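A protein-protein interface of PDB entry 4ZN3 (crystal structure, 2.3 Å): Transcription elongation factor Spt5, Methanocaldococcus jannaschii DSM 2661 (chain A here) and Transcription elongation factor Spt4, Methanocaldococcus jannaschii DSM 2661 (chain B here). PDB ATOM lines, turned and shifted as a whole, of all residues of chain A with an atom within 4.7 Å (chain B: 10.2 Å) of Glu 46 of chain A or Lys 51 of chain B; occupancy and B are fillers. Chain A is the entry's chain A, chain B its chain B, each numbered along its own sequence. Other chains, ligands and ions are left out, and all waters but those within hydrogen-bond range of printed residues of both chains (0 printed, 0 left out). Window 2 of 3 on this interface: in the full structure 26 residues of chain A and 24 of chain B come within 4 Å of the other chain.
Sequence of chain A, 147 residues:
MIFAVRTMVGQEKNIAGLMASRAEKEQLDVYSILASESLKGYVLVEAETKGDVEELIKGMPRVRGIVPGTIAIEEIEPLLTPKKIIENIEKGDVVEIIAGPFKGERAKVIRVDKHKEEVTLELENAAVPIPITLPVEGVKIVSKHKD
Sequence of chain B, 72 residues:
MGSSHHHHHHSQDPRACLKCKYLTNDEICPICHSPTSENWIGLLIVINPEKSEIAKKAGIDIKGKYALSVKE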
ATOM      1  N   MET A   1      19.374 -25.986  -0.419  1.00  0.00           N
ATOM      2  CA  MET A   1      18.305 -26.559  -1.294  1.00  0.00           C
ATOM      3  C   MET A   1      17.456 -27.551  -0.529  1.00  0.00           C
ATOM      4  O   MET A   1      17.949 -28.231   0.369  1.00  0.00           O
ATOM      5  CB  MET A   1      18.896 -27.256  -2.523  1.00  0.00           C
ATOM      6  CG  MET A   1      19.115 -26.340  -3.707  1.00  0.00           C
ATOM      7  SD  MET A   1      20.114 -27.154  -4.967  1.00  0.00           S
ATOM      8  CE  MET A   1      21.673 -26.291  -4.756  1.00  0.00           C
ATOM      9  N   ILE A   2      16.182 -27.630  -0.896  1.00  0.00           N
ATOM     10  CA  ILE A   2      15.237 -28.525  -0.243  1.00  0.00           C
ATOM     11  C   ILE A   2      14.574 -29.373  -1.310  1.00  0.00           C
ATOM     12  O   ILE A   2      14.200 -28.862  -2.364  1.00  0.00           O
ATOM     13  CB  ILE A   2      14.172 -27.745   0.551  1.00  0.00           C
ATOM     14  CG1 ILE A   2      14.848 -26.829   1.590  1.00  0.00           C
ATOM     15  CG2 ILE A   2      13.194 -28.703   1.225  1.00  0.00           C
ATOM     16  CD1 ILE A   2      14.047 -25.612   1.983  1.00  0.00           C
ATOM     17  N   ASP A  29      26.049 -33.517   3.450  1.00  0.00           N
ATOM     18  CA  ASP A  29      25.656 -32.121   3.665  1.00  0.00           C
ATOM     19  C   ASP A  29      24.135 -32.004   3.698  1.00  0.00           C
ATOM     20  O   ASP A  29      23.533 -31.390   2.821  1.00  0.00           O
ATOM     21  CB  ASP A  29      26.246 -31.224   2.574  1.00  0.00           C
ATOM     22  CG  ASP A  29      27.762 -31.249   2.552  1.00  0.00           C
ATOM     23  OD1 ASP A  29      28.376 -31.190   3.636  1.00  0.00           O
ATOM     24  OD2 ASP A  29      28.338 -31.318   1.445  1.00  0.00           O
ATOM     25  N   VAL A  30      23.536 -32.602   4.729  1.00  0.00           N
ATOM     26  CA  VAL A  30      22.087 -32.650   4.921  1.00  0.00           C
ATOM     27  C   VAL A  30      21.811 -31.900   6.215  1.00  0.00           C
ATOM     28  O   VAL A  30      22.291 -32.295   7.280  1.00  0.00           O
ATOM     29  CB  VAL A  30      21.580 -34.105   5.025  1.00  0.00           C
ATOM     30  CG1 VAL A  30      20.072 -34.151   5.245  1.00  0.00           C
ATOM     31  CG2 VAL A  30      21.950 -34.884   3.769  1.00  0.00           C
ATOM     32  N   TYR A  31      21.041 -30.823   6.116  1.00  0.00           N
ATOM     33  CA  TYR A  31      20.892 -29.866   7.213  1.00  0.00           C
ATOM     34  C   TYR A  31      19.601 -30.027   8.008  1.00  0.00           C
ATOM     35  O   TYR A  31      19.579 -29.740   9.201  1.00  0.00           O
ATOM     36  CB  TYR A  31      21.017 -28.435   6.677  1.00  0.00           C
ATOM     37  CG  TYR A  31      22.207 -28.230   5.764  1.00  0.00           C
ATOM     38  CD1 TYR A  31      23.461 -28.756   6.087  1.00  0.00           C
ATOM     39  CD2 TYR A  31      22.085 -27.506   4.574  1.00  0.00           C
ATOM     40  CE1 TYR A  31      24.552 -28.571   5.253  1.00  0.00           C
ATOM     41  CE2 TYR A  31      23.174 -27.312   3.736  1.00  0.00           C
ATOM     42  CZ  TYR A  31      24.402 -27.851   4.078  1.00  0.00           C
ATOM     43  OH  TYR A  31      25.490 -27.666   3.266  1.00  0.00           O
ATOM     44  N   SER A  32      18.530 -30.469   7.361  1.00  0.00           N
ATOM     45  CA  SER A  32      17.292 -30.768   8.075  1.00  0.00           C
ATOM     46  C   SER A  32      16.438 -31.744   7.314  1.00  0.00           C
ATOM     47  O   SER A  32      16.639 -31.967   6.124  1.00  0.00           O
ATOM     48  CB  SER A  32      16.497 -29.494   8.394  1.00  0.00           C
ATOM     49  OG  SER A  32      15.956 -28.897   7.228  1.00  0.00           O
ATOM     50  N   LEU A  44      10.645 -34.148   3.409  1.00  0.00           N
ATOM     51  CA  LEU A  44      11.435 -33.066   2.828  1.00  0.00           C
ATOM     52  C   LEU A  44      12.831 -33.095   3.421  1.00  0.00           C
ATOM     53  O   LEU A  44      12.982 -33.086   4.645  1.00  0.00           O
ATOM     54  CB  LEU A  44      10.786 -31.705   3.097  1.00  0.00           C
ATOM     55  CG  LEU A  44       9.351 -31.514   2.587  1.00  0.00           C
ATOM     56  CD1 LEU A  44       8.863 -30.109   2.899  1.00  0.00           C
ATOM     57  CD2 LEU A  44       9.248 -31.789   1.095  1.00  0.00           C
ATOM     58  N   VAL A  45      13.833 -33.121   2.547  1.00  0.00           N
ATOM     59  CA  VAL A  45      15.240 -33.173   2.932  1.00  0.00           C
ATOM     60  C   VAL A  45      15.933 -31.897   2.468  1.00  0.00           C
ATOM     61  O   VAL A  45      15.956 -31.602   1.272  1.00  0.00           O
ATOM     62  CB  VAL A  45      15.942 -34.386   2.288  1.00  0.00           C
ATOM     63  CG1 VAL A  45      17.405 -34.452   2.714  1.00  0.00           C
ATOM     64  CG2 VAL A  45      15.211 -35.673   2.644  1.00  0.00           C
ATOM     65  N   GLU A  46      16.496 -31.148   3.412  1.00  0.00           N
ATOM     66  CA  GLU A  46      17.285 -29.962   3.094  1.00  0.00           C
ATOM     67  C   GLU A  46      18.755 -30.342   2.995  1.00  0.00           C
ATOM     68  O   GLU A  46      19.324 -30.851   3.958  1.00  0.00           O
ATOM     69  CB  GLU A  46      17.101 -28.880   4.155  1.00  0.00           C
ATOM     70  CG  GLU A  46      17.793 -27.569   3.812  1.00  0.00           C
ATOM     71  CD  GLU A  46      17.628 -26.510   4.874  1.00  0.00           C
ATOM     72  OE1 GLU A  46      18.060 -25.372   4.624  1.00  0.00           O
ATOM     73  OE2 GLU A  46      17.080 -26.801   5.963  1.00  0.00           O
ATOM     74  N   ALA A  47      19.361 -30.083   1.838  1.00  0.00           N
ATOM     75  CA  ALA A  47      20.769 -30.405   1.596  1.00  0.00           C
ATOM     76  C   ALA A  47      21.448 -29.370   0.701  1.00  0.00           C
ATOM     77  O   ALA A  47      20.780 -28.543   0.069  1.00  0.00           O
ATOM     78  CB  ALA A  47      20.892 -31.797   0.983  1.00  0.00           C
ATOM     79  N   LEU B  44      10.360 -32.253  12.658  1.00  0.00           N
ATOM     80  CA  LEU B  44      11.456 -31.519  12.043  1.00  0.00           C
ATOM     81  C   LEU B  44      12.736 -31.972  12.727  1.00  0.00           C
ATOM     82  O   LEU B  44      12.902 -31.769  13.930  1.00  0.00           O
ATOM     83  CB  LEU B  44      11.263 -30.011  12.207  1.00  0.00           C
ATOM     84  CG  LEU B  44      12.376 -29.079  11.709  1.00  0.00           C
ATOM     85  CD1 LEU B  44      12.767 -29.353  10.263  1.00  0.00           C
ATOM     86  CD2 LEU B  44      11.944 -27.630  11.870  1.00  0.00           C
ATOM     87  N   ILE B  45      13.620 -32.611  11.963  1.00  0.00           N
ATOM     88  CA  ILE B  45      14.936 -33.004  12.457  1.00  0.00           C
ATOM     89  C   ILE B  45      15.937 -31.972  11.973  1.00  0.00           C
ATOM     90  O   ILE B  45      16.194 -31.872  10.777  1.00  0.00           O
ATOM     91  CB  ILE B  45      15.343 -34.412  11.973  1.00  0.00           C
ATOM     92  CG1 ILE B  45      14.292 -35.443  12.415  1.00  0.00           C
ATOM     93  CG2 ILE B  45      16.722 -34.780  12.513  1.00  0.00           C
ATOM     94  CD1 ILE B  45      14.580 -36.866  11.985  1.00  0.00           C
ATOM     95  N   VAL B  46      16.493 -31.208  12.909  1.00  0.00           N
ATOM     96  CA  VAL B  46      17.532 -30.233  12.607  1.00  0.00           C
ATOM     97  C   VAL B  46      18.875 -30.910  12.834  1.00  0.00           C
ATOM     98  O   VAL B  46      19.220 -31.239  13.971  1.00  0.00           O
ATOM     99  CB  VAL B  46      17.409 -28.974  13.495  1.00  0.00           C
ATOM    100  CG1 VAL B  46      18.514 -27.975  13.173  1.00  0.00           C
ATOM    101  CG2 VAL B  46      16.044 -28.335  13.297  1.00  0.00           C
ATOM    102  N   ILE B  47      19.616 -31.122  11.749  1.00  0.00           N
ATOM    103  CA  ILE B  47      20.938 -31.750  11.803  1.00  0.00           C
ATOM    104  C   ILE B  47      22.021 -30.683  11.933  1.00  0.00           C
ATOM    105  O   ILE B  47      22.917 -30.816  12.758  1.00  0.00           O
ATOM    106  CB  ILE B  47      21.191 -32.644  10.568  1.00  0.00           C
ATOM    107  CG1 ILE B  47      20.178 -33.797  10.550  1.00  0.00           C
ATOM    108  CG2 ILE B  47      22.611 -33.210  10.583  1.00  0.00           C
ATOM    109  CD1 ILE B  47      19.982 -34.427   9.195  1.00  0.00           C
ATOM    110  N   ASN B  48      21.928 -29.639  11.114  1.00  0.00           N
ATOM    111  CA  ASN B  48      22.867 -28.527  11.137  1.00  0.00           C
ATOM    112  C   ASN B  48      22.072 -27.223  11.248  1.00  0.00           C
ATOM    113  O   ASN B  48      21.640 -26.679  10.229  1.00  0.00           O
ATOM    114  CB  ASN B  48      23.729 -28.556   9.868  1.00  0.00           C
ATOM    115  CG  ASN B  48      24.882 -27.561   9.910  1.00  0.00           C
ATOM    116  OD1 ASN B  48      24.782 -26.496  10.512  1.00  0.00           O
ATOM    117  ND2 ASN B  48      25.978 -27.900   9.243  1.00  0.00           N
ATOM    118  N   PRO B  49      21.859 -26.724  12.482  1.00  0.00           N
ATOM    119  CA  PRO B  49      21.038 -25.511  12.643  1.00  0.00           C
ATOM    120  C   PRO B  49      21.564 -24.261  11.928  1.00  0.00           C
ATOM    121  O   PRO B  49      20.770 -23.486  11.400  1.00  0.00           O
ATOM    122  CB  PRO B  49      20.997 -25.286  14.170  1.00  0.00           C
ATOM    123  CG  PRO B  49      21.990 -26.221  14.759  1.00  0.00           C
ATOM    124  CD  PRO B  49      22.217 -27.327  13.779  1.00  0.00           C
ATOM    125  N   GLU B  50      22.881 -24.089  11.892  1.00  0.00           N
ATOM    126  CA  GLU B  50      23.485 -22.878  11.311  1.00  0.00           C
ATOM    127  C   GLU B  50      23.442 -22.851   9.780  1.00  0.00           C
ATOM    128  O   GLU B  50      23.493 -21.776   9.192  1.00  0.00           O
ATOM    129  CB  GLU B  50      24.915 -22.603  11.842  1.00  0.00           C
ATOM    130  CG  GLU B  50      25.893 -23.779  11.914  1.00  0.00           C
ATOM    131  CD  GLU B  50      25.730 -24.646  13.167  1.00  0.00           C
ATOM    132  OE1 GLU B  50      25.555 -24.095  14.276  1.00  0.00           O
ATOM    133  OE2 GLU B  50      25.764 -25.891  13.046  1.00  0.00           O
ATOM    134  N   LYS B  51      23.325 -24.018   9.144  1.00  0.00           N
ATOM    135  CA  LYS B  51      23.159 -24.099   7.690  1.00  0.00           C
ATOM    136  C   LYS B  51      21.716 -24.357   7.228  1.00  0.00           C
ATOM    137  O   LYS B  51      21.417 -24.165   6.051  1.00  0.00           O
ATOM    138  CB  LYS B  51      24.104 -25.155   7.112  1.00  0.00           C
ATOM    139  CG  LYS B  51      25.542 -24.667   6.999  1.00  0.00           C
ATOM    140  CD  LYS B  51      26.453 -25.738   6.426  1.00  0.00           C
ATOM    141  CE  LYS B  51      27.729 -25.158   5.835  1.00  0.00           C
ATOM    142  NZ  LYS B  51      28.572 -26.230   5.235  1.00  0.00           N
ATOM    143  N   SER B  52      20.831 -24.776   8.134  1.00  0.00           N
ATOM    144  CA  SER B  52      19.433 -25.058   7.779  1.00  0.00           C
ATOM    145  C   SER B  52      18.573 -23.788   7.775  1.00  0.00           C
ATOM    146  O   SER B  52      18.385 -23.158   8.821  1.00  0.00           O
ATOM    147  CB  SER B  52      18.831 -26.083   8.746  1.00  0.00           C
ATOM    148  OG  SER B  52      17.459 -26.311   8.473  1.00  0.00           O
ATOM    149  N   GLU B  53      18.050 -23.416   6.608  1.00  0.00           N
ATOM    150  CA  GLU B  53      17.070 -22.321   6.536  1.00  0.00           C
ATOM    151  C   GLU B  53      15.678 -22.748   7.024  1.00  0.00           C
ATOM    152  O   GLU B  53      14.896 -21.896   7.452  1.00  0.00           O
ATOM    153  CB  GLU B  53      17.004 -21.650   5.150  1.00  0.00           C
ATOM    154  CG  GLU B  53      16.804 -22.561   3.949  1.00  0.00           C
ATOM    155  CD  GLU B  53      16.553 -21.810   2.649  1.00  0.00           C
ATOM    156  OE1 GLU B  53      16.660 -22.453   1.580  1.00  0.00           O
ATOM    157  OE2 GLU B  53      16.253 -20.592   2.679  1.00  0.00           O
ATOM    158  N   ILE B  54      15.376 -24.051   6.985  1.00  0.00           N
ATOM    159  CA  ILE B  54      14.160 -24.562   7.632  1.00  0.00           C
ATOM    160  C   ILE B  54      14.231 -24.311   9.141  1.00  0.00           C
ATOM    161  O   ILE B  54      13.271 -23.825   9.733  1.00  0.00           O
ATOM    162  CB  ILE B  54      13.891 -26.062   7.344  1.00  0.00           C
ATOM    163  CG1 ILE B  54      13.672 -26.274   5.836  1.00  0.00           C
ATOM    164  CG2 ILE B  54      12.665 -26.543   8.123  1.00  0.00           C
ATOM    165  CD1 ILE B  54      13.308 -27.684   5.408  1.00  0.00           C
ATOM    166  N   ALA B  55      15.369 -24.633   9.746  1.00  0.00           N
ATOM    167  CA  ALA B  55      15.584 -24.393  11.176  1.00  0.00           C
ATOM    168  C   ALA B  55      15.557 -22.900  11.518  1.00  0.00           C
ATOM    169  O   ALA B  55      15.023 -22.512  12.560  1.00  0.00           O
ATOM    170  CB  ALA B  55      16.895 -25.016  11.622  1.00  0.00           C
ATOM    171  N   LYS B  56      16.125 -22.073  10.640  1.00  0.00           N
ATOM    172  CA  LYS B  56      16.060 -20.616  10.786  1.00  0.00           C
ATOM    173  C   LYS B  56      14.606 -20.148  10.807  1.00  0.00           C
ATOM    174  O   LYS B  56      14.208 -19.407  11.704  1.00  0.00           O
ATOM    175  CB  LYS B  56      16.821 -19.913   9.659  1.00  0.00           C
ATOM    176  N   LYS B  57      13.815 -20.614   9.842  1.00  0.00           N
ATOM    177  CA  LYS B  57      12.389 -20.274   9.780  1.00  0.00           C
ATOM    178  C   LYS B  57      11.597 -20.794  10.979  1.00  0.00           C
ATOM    179  O   LYS B  57      10.653 -20.147  11.418  1.00  0.00           O
ATOM    180  CB  LYS B  57      11.760 -20.791   8.487  1.00  0.00           C
ATOM    181  CG  LYS B  57      12.253 -20.087   7.236  1.00  0.00           C
ATOM    182  CD  LYS B  57      11.612 -18.722   7.043  1.00  0.00           C
ATOM    183  CE  LYS B  57      12.255 -17.998   5.872  1.00  0.00           C
ATOM    184  NZ  LYS B  57      11.455 -16.827   5.431  1.00  0.00           N
ATOM    185  N   ALA B  58      11.984 -21.957  11.500  1.00  0.00           N
ATOM    186  CA  ALA B  58      11.333 -22.547  12.671  1.00  0.00           C
ATOM    187  C   ALA B  58      11.766 -21.917  13.997  1.00  0.00           C
ATOM    188  O   ALA B  58      11.166 -22.205  15.031  1.00  0.00           O
ATOM    189  CB  ALA B  58      11.584 -24.048  12.707  1.00  0.00           C
ATOM    190  N   ILE B  60      14.777 -22.459  15.351  1.00  0.00           N
ATOM    191  CA  ILE B  60      15.516 -23.515  16.039  1.00  0.00           C
ATOM    192  C   ILE B  60      17.012 -23.319  15.796  1.00  0.00           C
ATOM    193  O   ILE B  60      17.461 -23.337  14.649  1.00  0.00           O
ATOM    194  CB  ILE B  60      15.079 -24.914  15.553  1.00  0.00           C
ATOM    195  CG1 ILE B  60      13.610 -25.164  15.937  1.00  0.00           C
ATOM    196  CG2 ILE B  60      15.984 -25.996  16.144  1.00  0.00           C
ATOM    197  CD1 ILE B  60      12.974 -26.371  15.274  1.00  0.00           C
ATOM    198  N   ASP B  61      17.768 -23.141  16.881  1.00  0.00           N
ATOM    199  CA  ASP B  61      19.222 -22.998  16.817  1.00  0.00           C
ATOM    200  C   ASP B  61      19.991 -24.140  17.510  1.00  0.00           C
ATOM    201  O   ASP B  61      21.214 -24.094  17.568  1.00  0.00           O
ATOM    202  CB  ASP B  61      19.649 -21.621  17.372  1.00  0.00           C
ATOM    203  CG  ASP B  61      19.447 -21.481  18.886  1.00  0.00           C
ATOM    204  OD1 ASP B  61      18.921 -22.408  19.543  1.00  0.00           O
ATOM    205  OD2 ASP B  61      19.812 -20.417  19.432  1.00  0.00           O
ATOM    206  N   ILE B  62      19.287 -25.151  18.026  1.00  0.00           N
ATOM    207  CA  ILE B  62      19.921 -26.315  18.658  1.00  0.00           C
ATOM    208  C   ILE B  62      19.528 -27.571  17.888  1.00  0.00           C
ATOM    209  O   ILE B  62      18.344 -27.790  17.618  1.00  0.00           O
ATOM    210  CB  ILE B  62      19.505 -26.460  20.142  1.00  0.00           C
ATOM    211  CG1 ILE B  62      20.093 -25.312  20.973  1.00  0.00           C
ATOM    212  CG2 ILE B  62      19.975 -27.800  20.723  1.00  0.00           C
ATOM    213  CD1 ILE B  62      19.400 -25.111  22.304  1.00  0.00           C
ATOM    214  N   LYS B  63      20.512 -28.405  17.560  1.00  0.00           N
ATOM    215  CA  LYS B  63      20.256 -29.592  16.753  1.00  0.00           C
ATOM    216  C   LYS B  63      19.469 -30.618  17.559  1.00  0.00           C
ATOM    217  O   LYS B  63      19.629 -30.722  18.775  1.00  0.00           O
ATOM    218  CB  LYS B  63      21.552 -30.183  16.187  1.00  0.00           C
ATOM    219  CG  LYS B  63      22.339 -31.101  17.108  1.00  0.00           C
ATOM    220  CD  LYS B  63      23.590 -31.622  16.415  1.00  0.00           C
ATOM    221  CE  LYS B  63      23.272 -32.751  15.442  1.00  0.00           C
ATOM    222  NZ  LYS B  63      24.440 -33.102  14.588  1.00  0.00           N
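The backbone NH (N) of Ile 47 of chain B is in hydrogen-bond range of the backbone carbonyl oxygen (O) of Tyr 31 of chain A (2.9 Å).
The backbone carbonyl oxygen of Tyr 31 of chain A lies within hydrogen-bond range of the backbone NH of Asn 48 of chain B (3.0 Å).
OG of Ser 52 of chain B lies within hydrogen-bond range of OG of Ser 32 of chain A, at 3.2 Å.
OE2 of Glu 46 of chain A lies within hydrogen-bond range of OG of Ser 52 of chain B, at 2.6 Å.
OE1 of Glu 46 of chain A sits at hydrogen-bond distance from N of Glu 53 of chain B, 2.8 Å away.
N of Ile 54 of chain B sits at hydrogen-bond distance from OE2 of Glu 46 of chain A (3.4 Å).
Met 1 of chain A touches none of the printed residues of chain B.
Of the printed residues of chain B, Ile 2 of chain A touches Ile 54 (3.9 Å).
Of the printed residues of chain B, Val 30 of chain A touches Ile 47 (3.4 Å).
Of chain B, only Val 46, Ile 47, Asn 48, Lys 51 and Ser 52 come within 4 Å of Tyr 31 of chain A.
Of chain B, only Ile 45, Ser 52 and Ile 54 come within 4 Å of Ser 32 of chain A.
No residue of chain B comes within 4 Å of Val 45 of chain A.
Printed residues of chain B within 4 Å of Glu 46 of chain A: Lys 51 (3.8 Å), Ser 52 (2.6 Å), Glu 53 (2.8 Å) and Ile 54 (3.4 Å).
Ala 47 of chain A touches none of the printed residues of chain B.
Of the printed residues of chain A, Ile 45 of chain B touches Ser 32 (3.1 Å).
Of the printed residues of chain A, Ile 47 of chain B touches Val 30 (3.4 Å) and Tyr 31 (2.9 Å).
Lys 51 of chain B touches just these residues of chain A: Tyr 31 and Glu 46.
Printed residues of chain A within 4 Å of Ser 52 of chain B: Tyr 31, Ser 32 and Glu 46.
Of the printed residues of chain A, Glu 53 of chain B touches Glu 46 (2.8 Å).
Lys 57 of chain B touches none of the printed residues of chain A.
The nearest printed residue of chain A that does not touch Lys 51 of chain B is Asp 29 of chain A (5.2 Å).
The nearest printed residue of chain A that does not touch Val 46 of chain B is Ser 32 of chain A (4.4 Å).
OE2 of Glu 46 of chain A sits at hydrogen-bond distance from OG of Ser 32 of chain A (2.7 Å).
NZ of Lys 63 of chain B lies within hydrogen-bond range of O of Ile 47 of chain B (3.3 Å).
The side-chain amide oxygen (OD1) of Asn 48 of chain B lies close to the side-chain carboxylate (OE2) of Glu 50 of chain B, at 2.8 Å.
The backbone NH (N) of Lys 51 of chain B lies within hydrogen-bond range of the side-chain amide oxygen (OD1) of Asn 48 of chain B, 3.2 Å away.
The side-chain hydroxyl (OG) of Ser 52 of chain B lies close to the backbone NH (N) of Ile 54 of chain B (3.4 Å).
The side-chain hydroxyl (OG) of Ser 52 of chain B is in hydrogen-bond range of the backbone NH (N) of Ala 55 of chain B (3.0 Å).
Among the printed residues, merely in contact across the chains: Ser 32 of chain A with Ile 45 of chain B (3.1 Å), Ser 32 of chain A with Ile 54 of chain B (3.4 Å), Val 30 of chain A with Ile 47 of chain B (3.4 Å), Tyr 31 of chain A with Lys 51 of chain B (3.6 Å), Tyr 31 of chain A with Ser 52 of chain B (3.8 Å), Glu 46 of chain A with Lys 51 of chain B (3.8 Å), Tyr 31 of chain A with Val 46 of chain B (3.9 Å) and Ile 2 of chain A with Ile 54 of chain B (3.9 Å).
Printed residues of chain A that touch a printed residue of chain B: Ile 2, Val 30, Tyr 31, Ser 32 and Glu 46.
Printed residues of chain B that touch a printed residue of chain A: Ile 45, Val 46, Ile 47, Asn 48, Lys 51, Ser 52, Glu 53 and Ile 54.
Among the printed residues, 14 pairs touch across the chains.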
